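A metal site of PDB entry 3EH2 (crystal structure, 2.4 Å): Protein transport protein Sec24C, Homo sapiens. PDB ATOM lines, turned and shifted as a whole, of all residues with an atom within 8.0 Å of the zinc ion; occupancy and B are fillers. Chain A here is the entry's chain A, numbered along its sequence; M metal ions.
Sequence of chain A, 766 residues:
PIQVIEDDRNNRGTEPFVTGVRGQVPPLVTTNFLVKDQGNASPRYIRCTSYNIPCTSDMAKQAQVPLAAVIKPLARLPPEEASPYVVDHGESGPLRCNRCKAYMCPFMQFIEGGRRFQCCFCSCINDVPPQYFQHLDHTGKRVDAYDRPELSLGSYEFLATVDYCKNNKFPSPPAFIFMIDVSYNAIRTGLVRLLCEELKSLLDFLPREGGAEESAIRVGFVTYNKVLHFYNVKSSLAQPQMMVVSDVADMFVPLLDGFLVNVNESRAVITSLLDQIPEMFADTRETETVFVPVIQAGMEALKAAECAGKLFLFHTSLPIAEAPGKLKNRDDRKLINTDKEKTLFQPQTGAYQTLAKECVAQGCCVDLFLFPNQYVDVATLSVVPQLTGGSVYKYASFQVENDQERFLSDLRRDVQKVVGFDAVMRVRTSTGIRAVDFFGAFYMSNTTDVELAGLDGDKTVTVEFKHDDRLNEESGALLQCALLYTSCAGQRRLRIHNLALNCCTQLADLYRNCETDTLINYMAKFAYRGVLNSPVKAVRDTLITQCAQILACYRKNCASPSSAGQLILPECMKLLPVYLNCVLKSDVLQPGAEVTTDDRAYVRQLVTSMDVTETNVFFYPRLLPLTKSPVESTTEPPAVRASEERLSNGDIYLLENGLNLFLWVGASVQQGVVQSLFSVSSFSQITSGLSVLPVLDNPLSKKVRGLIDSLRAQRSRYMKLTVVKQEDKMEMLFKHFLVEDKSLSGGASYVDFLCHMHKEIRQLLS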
ATOM      1  N   ARG A  96     -22.081  -8.897  -7.134  1.00  0.00           N
ATOM      2  CA  ARG A  96     -21.449 -10.129  -7.572  1.00  0.00           C
ATOM      3  C   ARG A  96     -20.596  -9.898  -8.813  1.00  0.00           C
ATOM      4  O   ARG A  96     -20.765  -8.913  -9.518  1.00  0.00           O
ATOM      5  CB  ARG A  96     -22.528 -11.175  -7.905  1.00  0.00           C
ATOM      6  CG  ARG A  96     -23.584 -11.369  -6.817  1.00  0.00           C
ATOM      7  CD  ARG A  96     -24.711 -12.338  -7.240  1.00  0.00           C
ATOM      8  NE  ARG A  96     -24.203 -13.663  -7.586  1.00  0.00           N
ATOM      9  CZ  ARG A  96     -24.979 -14.692  -7.951  1.00  0.00           C
ATOM     10  NH1 ARG A  96     -26.287 -14.548  -8.035  1.00  0.00           N
ATOM     11  NH2 ARG A  96     -24.431 -15.875  -8.221  1.00  0.00           N
ATOM     12  N   CYS A  97     -19.653 -10.804  -9.061  1.00  0.00           N
ATOM     13  CA  CYS A  97     -18.809 -10.644 -10.229  1.00  0.00           C
ATOM     14  C   CYS A  97     -19.683 -10.794 -11.477  1.00  0.00           C
ATOM     15  O   CYS A  97     -20.383 -11.797 -11.660  1.00  0.00           O
ATOM     16  CB  CYS A  97     -17.693 -11.663 -10.263  1.00  0.00           C
ATOM     17  SG  CYS A  97     -16.796 -11.602 -11.836  1.00  0.00           S
ATOM     18  N   ASN A  98     -19.629  -9.782 -12.330  1.00  0.00           N
ATOM     19  CA  ASN A  98     -20.415  -9.754 -13.549  1.00  0.00           C
ATOM     20  C   ASN A  98     -20.112 -10.917 -14.482  1.00  0.00           C
ATOM     21  O   ASN A  98     -20.950 -11.289 -15.307  1.00  0.00           O
ATOM     22  CB  ASN A  98     -20.170  -8.426 -14.251  1.00  0.00           C
ATOM     23  CG  ASN A  98     -21.013  -8.254 -15.484  1.00  0.00           C
ATOM     24  OD1 ASN A  98     -22.231  -8.429 -15.442  1.00  0.00           O
ATOM     25  ND2 ASN A  98     -20.376  -7.898 -16.587  1.00  0.00           N
ATOM     26  N   ARG A  99     -18.928 -11.508 -14.348  1.00  0.00           N
ATOM     27  CA  ARG A  99     -18.558 -12.629 -15.196  1.00  0.00           C
ATOM     28  C   ARG A  99     -18.789 -13.995 -14.559  1.00  0.00           C
ATOM     29  O   ARG A  99     -19.618 -14.764 -15.045  1.00  0.00           O
ATOM     30  CB  ARG A  99     -17.078 -12.536 -15.619  1.00  0.00           C
ATOM     31  CG  ARG A  99     -16.650 -13.712 -16.515  1.00  0.00           C
ATOM     32  CD  ARG A  99     -15.154 -13.686 -16.826  1.00  0.00           C
ATOM     33  NE  ARG A  99     -14.770 -12.457 -17.501  1.00  0.00           N
ATOM     34  CZ  ARG A  99     -13.525 -11.980 -17.532  1.00  0.00           C
ATOM     35  NH1 ARG A  99     -12.555 -12.637 -16.905  1.00  0.00           N
ATOM     36  NH2 ARG A  99     -13.263 -10.850 -18.186  1.00  0.00           N
ATOM     37  N   CYS A 100     -18.074 -14.310 -13.489  1.00  0.00           N
ATOM     38  CA  CYS A 100     -18.230 -15.621 -12.846  1.00  0.00           C
ATOM     39  C   CYS A 100     -19.343 -15.680 -11.791  1.00  0.00           C
ATOM     40  O   CYS A 100     -19.667 -16.748 -11.286  1.00  0.00           O
ATOM     41  CB  CYS A 100     -16.906 -16.059 -12.218  1.00  0.00           C
ATOM     42  SG  CYS A 100     -16.529 -15.261 -10.640  1.00  0.00           S
ATOM     43  N   LYS A 101     -19.899 -14.518 -11.448  1.00  0.00           N
ATOM     44  CA  LYS A 101     -20.983 -14.421 -10.458  1.00  0.00           C
ATOM     45  C   LYS A 101     -20.613 -14.751  -9.023  1.00  0.00           C
ATOM     46  O   LYS A 101     -21.486 -15.126  -8.237  1.00  0.00           O
ATOM     47  CB  LYS A 101     -22.188 -15.275 -10.886  1.00  0.00           C
ATOM     48  CG  LYS A 101     -22.855 -14.791 -12.164  1.00  0.00           C
ATOM     49  CD  LYS A 101     -24.082 -15.633 -12.510  1.00  0.00           C
ATOM     50  CE  LYS A 101     -25.231 -15.411 -11.525  1.00  0.00           C
ATOM     51  NZ  LYS A 101     -26.399 -16.317 -11.767  1.00  0.00           N
ATOM     52  N   ALA A 102     -19.335 -14.631  -8.673  1.00  0.00           N
ATOM     53  CA  ALA A 102     -18.900 -14.873  -7.303  1.00  0.00           C
ATOM     54  C   ALA A 102     -19.410 -13.677  -6.502  1.00  0.00           C
ATOM     55  O   ALA A 102     -19.561 -12.582  -7.058  1.00  0.00           O
ATOM     56  CB  ALA A 102     -17.385 -14.945  -7.231  1.00  0.00           C
ATOM     57  N   TYR A 103     -19.677 -13.869  -5.222  1.00  0.00           N
ATOM     58  CA  TYR A 103     -20.178 -12.782  -4.384  1.00  0.00           C
ATOM     59  C   TYR A 103     -19.046 -11.961  -3.784  1.00  0.00           C
ATOM     60  O   TYR A 103     -17.936 -12.463  -3.593  1.00  0.00           O
ATOM     61  CB  TYR A 103     -21.057 -13.354  -3.264  1.00  0.00           C
ATOM     62  CG  TYR A 103     -22.281 -14.113  -3.742  1.00  0.00           C
ATOM     63  CD1 TYR A 103     -23.526 -13.490  -3.847  1.00  0.00           C
ATOM     64  CD2 TYR A 103     -22.180 -15.452  -4.159  1.00  0.00           C
ATOM     65  CE1 TYR A 103     -24.646 -14.181  -4.353  1.00  0.00           C
ATOM     66  CE2 TYR A 103     -23.281 -16.148  -4.662  1.00  0.00           C
ATOM     67  CZ  TYR A 103     -24.512 -15.506  -4.759  1.00  0.00           C
ATOM     68  OH  TYR A 103     -25.585 -16.217  -5.262  1.00  0.00           O
ATOM     69  N   MET A 108     -11.940  -9.937  -2.644  1.00  0.00           N
ATOM     70  CA  MET A 108     -12.029  -9.068  -3.798  1.00  0.00           C
ATOM     71  C   MET A 108     -11.010  -7.927  -3.638  1.00  0.00           C
ATOM     72  O   MET A 108     -10.879  -7.336  -2.558  1.00  0.00           O
ATOM     73  CB  MET A 108     -13.457  -8.514  -3.960  1.00  0.00           C
ATOM     74  CG  MET A 108     -14.501  -9.583  -4.284  1.00  0.00           C
ATOM     75  SD  MET A 108     -14.159 -10.601  -5.741  1.00  0.00           S
ATOM     76  CE  MET A 108     -15.717 -11.424  -5.969  1.00  0.00           C
ATOM     77  N   PHE A 117     -13.437  -3.113  -8.644  1.00  0.00           N
ATOM     78  CA  PHE A 117     -12.783  -4.187  -7.908  1.00  0.00           C
ATOM     79  C   PHE A 117     -12.452  -5.290  -8.916  1.00  0.00           C
ATOM     80  O   PHE A 117     -13.203  -5.518  -9.860  1.00  0.00           O
ATOM     81  CB  PHE A 117     -13.669  -4.726  -6.765  1.00  0.00           C
ATOM     82  CG  PHE A 117     -14.791  -5.647  -7.214  1.00  0.00           C
ATOM     83  CD1 PHE A 117     -14.552  -7.016  -7.403  1.00  0.00           C
ATOM     84  CD2 PHE A 117     -16.084  -5.156  -7.389  1.00  0.00           C
ATOM     85  CE1 PHE A 117     -15.593  -7.876  -7.760  1.00  0.00           C
ATOM     86  CE2 PHE A 117     -17.132  -6.000  -7.749  1.00  0.00           C
ATOM     87  CZ  PHE A 117     -16.892  -7.362  -7.932  1.00  0.00           C
ATOM     88  N   GLN A 118     -11.307  -5.918  -8.733  1.00  0.00           N
ATOM     89  CA  GLN A 118     -10.903  -6.998  -9.602  1.00  0.00           C
ATOM     90  C   GLN A 118     -11.380  -8.271  -8.930  1.00  0.00           C
ATOM     91  O   GLN A 118     -11.148  -8.447  -7.731  1.00  0.00           O
ATOM     92  CB  GLN A 118      -9.392  -7.008  -9.762  1.00  0.00           C
ATOM     93  CG  GLN A 118      -8.879  -8.011 -10.782  1.00  0.00           C
ATOM     94  CD  GLN A 118      -7.383  -7.916 -10.957  1.00  0.00           C
ATOM     95  OE1 GLN A 118      -6.840  -8.305 -11.983  1.00  0.00           O
ATOM     96  NE2 GLN A 118      -6.703  -7.401  -9.944  1.00  0.00           N
ATOM     97  N   CYS A 119     -12.069  -9.133  -9.663  1.00  0.00           N
ATOM     98  CA  CYS A 119     -12.551 -10.368  -9.082  1.00  0.00           C
ATOM     99  C   CYS A 119     -11.384 -11.315  -8.799  1.00  0.00           C
ATOM    100  O   CYS A 119     -10.598 -11.638  -9.707  1.00  0.00           O
ATOM    101  CB  CYS A 119     -13.545 -11.038 -10.004  1.00  0.00           C
ATOM    102  SG  CYS A 119     -14.147 -12.571  -9.319  1.00  0.00           S
ATOM    103  N   CYS A 120     -11.277 -11.772  -7.563  1.00  0.00           N
ATOM    104  CA  CYS A 120     -10.178 -12.649  -7.170  1.00  0.00           C
ATOM    105  C   CYS A 120     -10.313 -14.052  -7.739  1.00  0.00           C
ATOM    106  O   CYS A 120      -9.336 -14.798  -7.807  1.00  0.00           O
ATOM    107  CB  CYS A 120     -10.106 -12.723  -5.655  1.00  0.00           C
ATOM    108  SG  CYS A 120     -11.676 -13.233  -4.892  1.00  0.00           S
ATOM    109  N   PHE A 121     -11.518 -14.408  -8.156  1.00  0.00           N
ATOM    110  CA  PHE A 121     -11.764 -15.730  -8.703  1.00  0.00           C
ATOM    111  C   PHE A 121     -11.512 -15.867 -10.197  1.00  0.00           C
ATOM    112  O   PHE A 121     -10.933 -16.866 -10.629  1.00  0.00           O
ATOM    113  CB  PHE A 121     -13.206 -16.185  -8.381  1.00  0.00           C
ATOM    114  CG  PHE A 121     -13.525 -16.172  -6.904  1.00  0.00           C
ATOM    115  CD1 PHE A 121     -14.185 -15.089  -6.330  1.00  0.00           C
ATOM    116  CD2 PHE A 121     -13.154 -17.227  -6.086  1.00  0.00           C
ATOM    117  CE1 PHE A 121     -14.470 -15.057  -4.958  1.00  0.00           C
ATOM    118  CE2 PHE A 121     -13.430 -17.212  -4.725  1.00  0.00           C
ATOM    119  CZ  PHE A 121     -14.090 -16.130  -4.151  1.00  0.00           C
ATOM    120  N   CYS A 122     -11.924 -14.872 -10.985  1.00  0.00           N
ATOM    121  CA  CYS A 122     -11.729 -14.948 -12.438  1.00  0.00           C
ATOM    122  C   CYS A 122     -11.012 -13.734 -13.014  1.00  0.00           C
ATOM    123  O   CYS A 122     -10.747 -13.667 -14.221  1.00  0.00           O
ATOM    124  CB  CYS A 122     -13.061 -15.098 -13.139  1.00  0.00           C
ATOM    125  SG  CYS A 122     -13.927 -13.530 -13.307  1.00  0.00           S
ATOM    126  N   SER A 123     -10.731 -12.767 -12.151  1.00  0.00           N
ATOM    127  CA  SER A 123     -10.022 -11.532 -12.500  1.00  0.00           C
ATOM    128  C   SER A 123     -10.800 -10.547 -13.353  1.00  0.00           C
ATOM    129  O   SER A 123     -10.236  -9.592 -13.885  1.00  0.00           O
ATOM    130  CB  SER A 123      -8.673 -11.853 -13.181  1.00  0.00           C
ATOM    131  OG  SER A 123      -8.836 -11.995 -14.582  1.00  0.00           O
ATOM    132  N   CYS A 124     -12.106 -10.752 -13.487  1.00  0.00           N
ATOM    133  CA  CYS A 124     -12.924  -9.823 -14.254  1.00  0.00           C
ATOM    134  C   CYS A 124     -12.954  -8.507 -13.469  1.00  0.00           C
ATOM    135  O   CYS A 124     -12.973  -8.531 -12.243  1.00  0.00           O
ATOM    136  CB  CYS A 124     -14.342 -10.354 -14.424  1.00  0.00           C
ATOM    137  SG  CYS A 124     -15.462  -9.222 -15.329  1.00  0.00           S
ATOM    138  N   ILE A 125     -12.940  -7.379 -14.191  1.00  0.00           N
ATOM    139  CA  ILE A 125     -12.995  -6.061 -13.548  1.00  0.00           C
ATOM    140  C   ILE A 125     -14.465  -5.649 -13.439  1.00  0.00           C
ATOM    141  O   ILE A 125     -15.219  -5.777 -14.410  1.00  0.00           O
ATOM    142  CB  ILE A 125     -12.247  -4.992 -14.360  1.00  0.00           C
ATOM    143  CG1 ILE A 125     -10.789  -5.427 -14.598  1.00  0.00           C
ATOM    144  CG2 ILE A 125     -12.272  -3.680 -13.603  1.00  0.00           C
ATOM    145  CD1 ILE A 125      -9.994  -5.599 -13.331  1.00  0.00           C
ATOM    146  N   ASN A 126     -14.867  -5.166 -12.271  1.00  0.00           N
ATOM    147  CA  ASN A 126     -16.247  -4.795 -12.027  1.00  0.00           C
ATOM    148  C   ASN A 126     -16.401  -3.436 -11.362  1.00  0.00           C
ATOM    149  O   ASN A 126     -15.615  -3.068 -10.480  1.00  0.00           O
ATOM    150  CB  ASN A 126     -16.902  -5.834 -11.117  1.00  0.00           C
ATOM    151  CG  ASN A 126     -17.023  -7.189 -11.762  1.00  0.00           C
ATOM    152  OD1 ASN A 126     -18.025  -7.490 -12.406  1.00  0.00           O
ATOM    153  ND2 ASN A 126     -15.992  -8.018 -11.609  1.00  0.00           N
ATOM    154  N   ARG A 428     -17.639 -21.979  -6.069  1.00  0.00           N
ATOM    155  CA  ARG A 428     -16.831 -21.323  -7.095  1.00  0.00           C
ATOM    156  C   ARG A 428     -15.368 -21.333  -6.620  1.00  0.00           C
ATOM    157  O   ARG A 428     -15.086 -21.295  -5.417  1.00  0.00           O
ATOM    158  CB  ARG A 428     -17.330 -19.895  -7.331  1.00  0.00           C
ATOM    159  CG  ARG A 428     -18.678 -19.842  -8.088  1.00  0.00           C
ATOM    160  CD  ARG A 428     -19.278 -18.451  -8.112  1.00  0.00           C
ATOM    161  NE  ARG A 428     -20.599 -18.445  -8.736  1.00  0.00           N
ATOM    162  CZ  ARG A 428     -21.741 -18.707  -8.108  1.00  0.00           C
ATOM    163  NH1 ARG A 428     -21.752 -18.998  -6.812  1.00  0.00           N
ATOM    164  NH2 ARG A 428     -22.878 -18.714  -8.781  1.00  0.00           N
ATOM    165  N   THR A 429     -14.438 -21.381  -7.561  1.00  0.00           N
ATOM    166  CA  THR A 429     -13.028 -21.418  -7.221  1.00  0.00           C
ATOM    167  C   THR A 429     -12.243 -20.474  -8.106  1.00  0.00           C
ATOM    168  O   THR A 429     -12.754 -20.000  -9.120  1.00  0.00           O
ATOM    169  CB  THR A 429     -12.470 -22.834  -7.447  1.00  0.00           C
ATOM    170  OG1 THR A 429     -12.675 -23.211  -8.811  1.00  0.00           O
ATOM    171  CG2 THR A 429     -13.190 -23.824  -6.574  1.00  0.00           C
ATOM    172  N   THR A 431      -9.859 -19.365 -10.991  1.00  0.00           N
ATOM    173  CA  THR A 431      -9.577 -19.968 -12.285  1.00  0.00           C
ATOM    174  C   THR A 431      -8.361 -20.893 -12.126  1.00  0.00           C
ATOM    175  O   THR A 431      -7.362 -20.507 -11.523  1.00  0.00           O
ATOM    176  CB  THR A 431      -9.273 -18.869 -13.361  1.00  0.00           C
ATOM    177  OG1 THR A 431     -10.446 -18.059 -13.556  1.00  0.00           O
ATOM    178  CG2 THR A 431      -8.886 -19.508 -14.699  1.00  0.00           C
HETATM  179 ZN    ZN M   1     -15.300 -13.304 -11.298  1.00  0.00          ZN
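Of the 22 residues printed, 4 come within 4 Å of the zinc ion. Along chain A the residues within 4 Å of the zinc ion span positions 97 to 122. The nearest printed residue that does not touch the zinc ion is Cys 124 (4.4 Å).
SG of Cys 97 binds the zinc ion (2.3 Å). The side-chain sulfur (SG) of Cys 100 binds the zinc ion, 2.4 Å away. The side-chain sulfur (SG) of Cys 119 is bound to the zinc ion (2.4 Å). SG of Cys 122 is bound to the zinc ion, 2.4 Å away.
The backbone carbonyl oxygen (O) of Cys 100 sits at hydrogen-bond distance from the guanidinium group (NE) of Arg 428 (3.2 Å). The backbone NH (N) of Cys 97 lies within hydrogen-bond range of the backbone carbonyl oxygen (O) of Ala 102 (2.7 Å). NH1 of Arg 99 is in hydrogen-bond range of O of Cys 122 (3.4 Å). The side-chain sulfur (SG) of Cys 100 lies close to the backbone NH (N) of Ala 102, 3.5 Å away. The side-chain amide nitrogen of Asn 126 lies close to the side-chain sulfur of Cys 97, at 3.7 Å. The backbone NH of Arg 99 lies close to the side-chain sulfur of Cys 97 (3.3 Å). The side-chain sulfur of Cys 119 lies close to the backbone NH of Phe 121. The backbone NH (N) of Cys 119 is in hydrogen-bond range of the backbone carbonyl oxygen (O) of Cys 124, 2.8 Å away.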
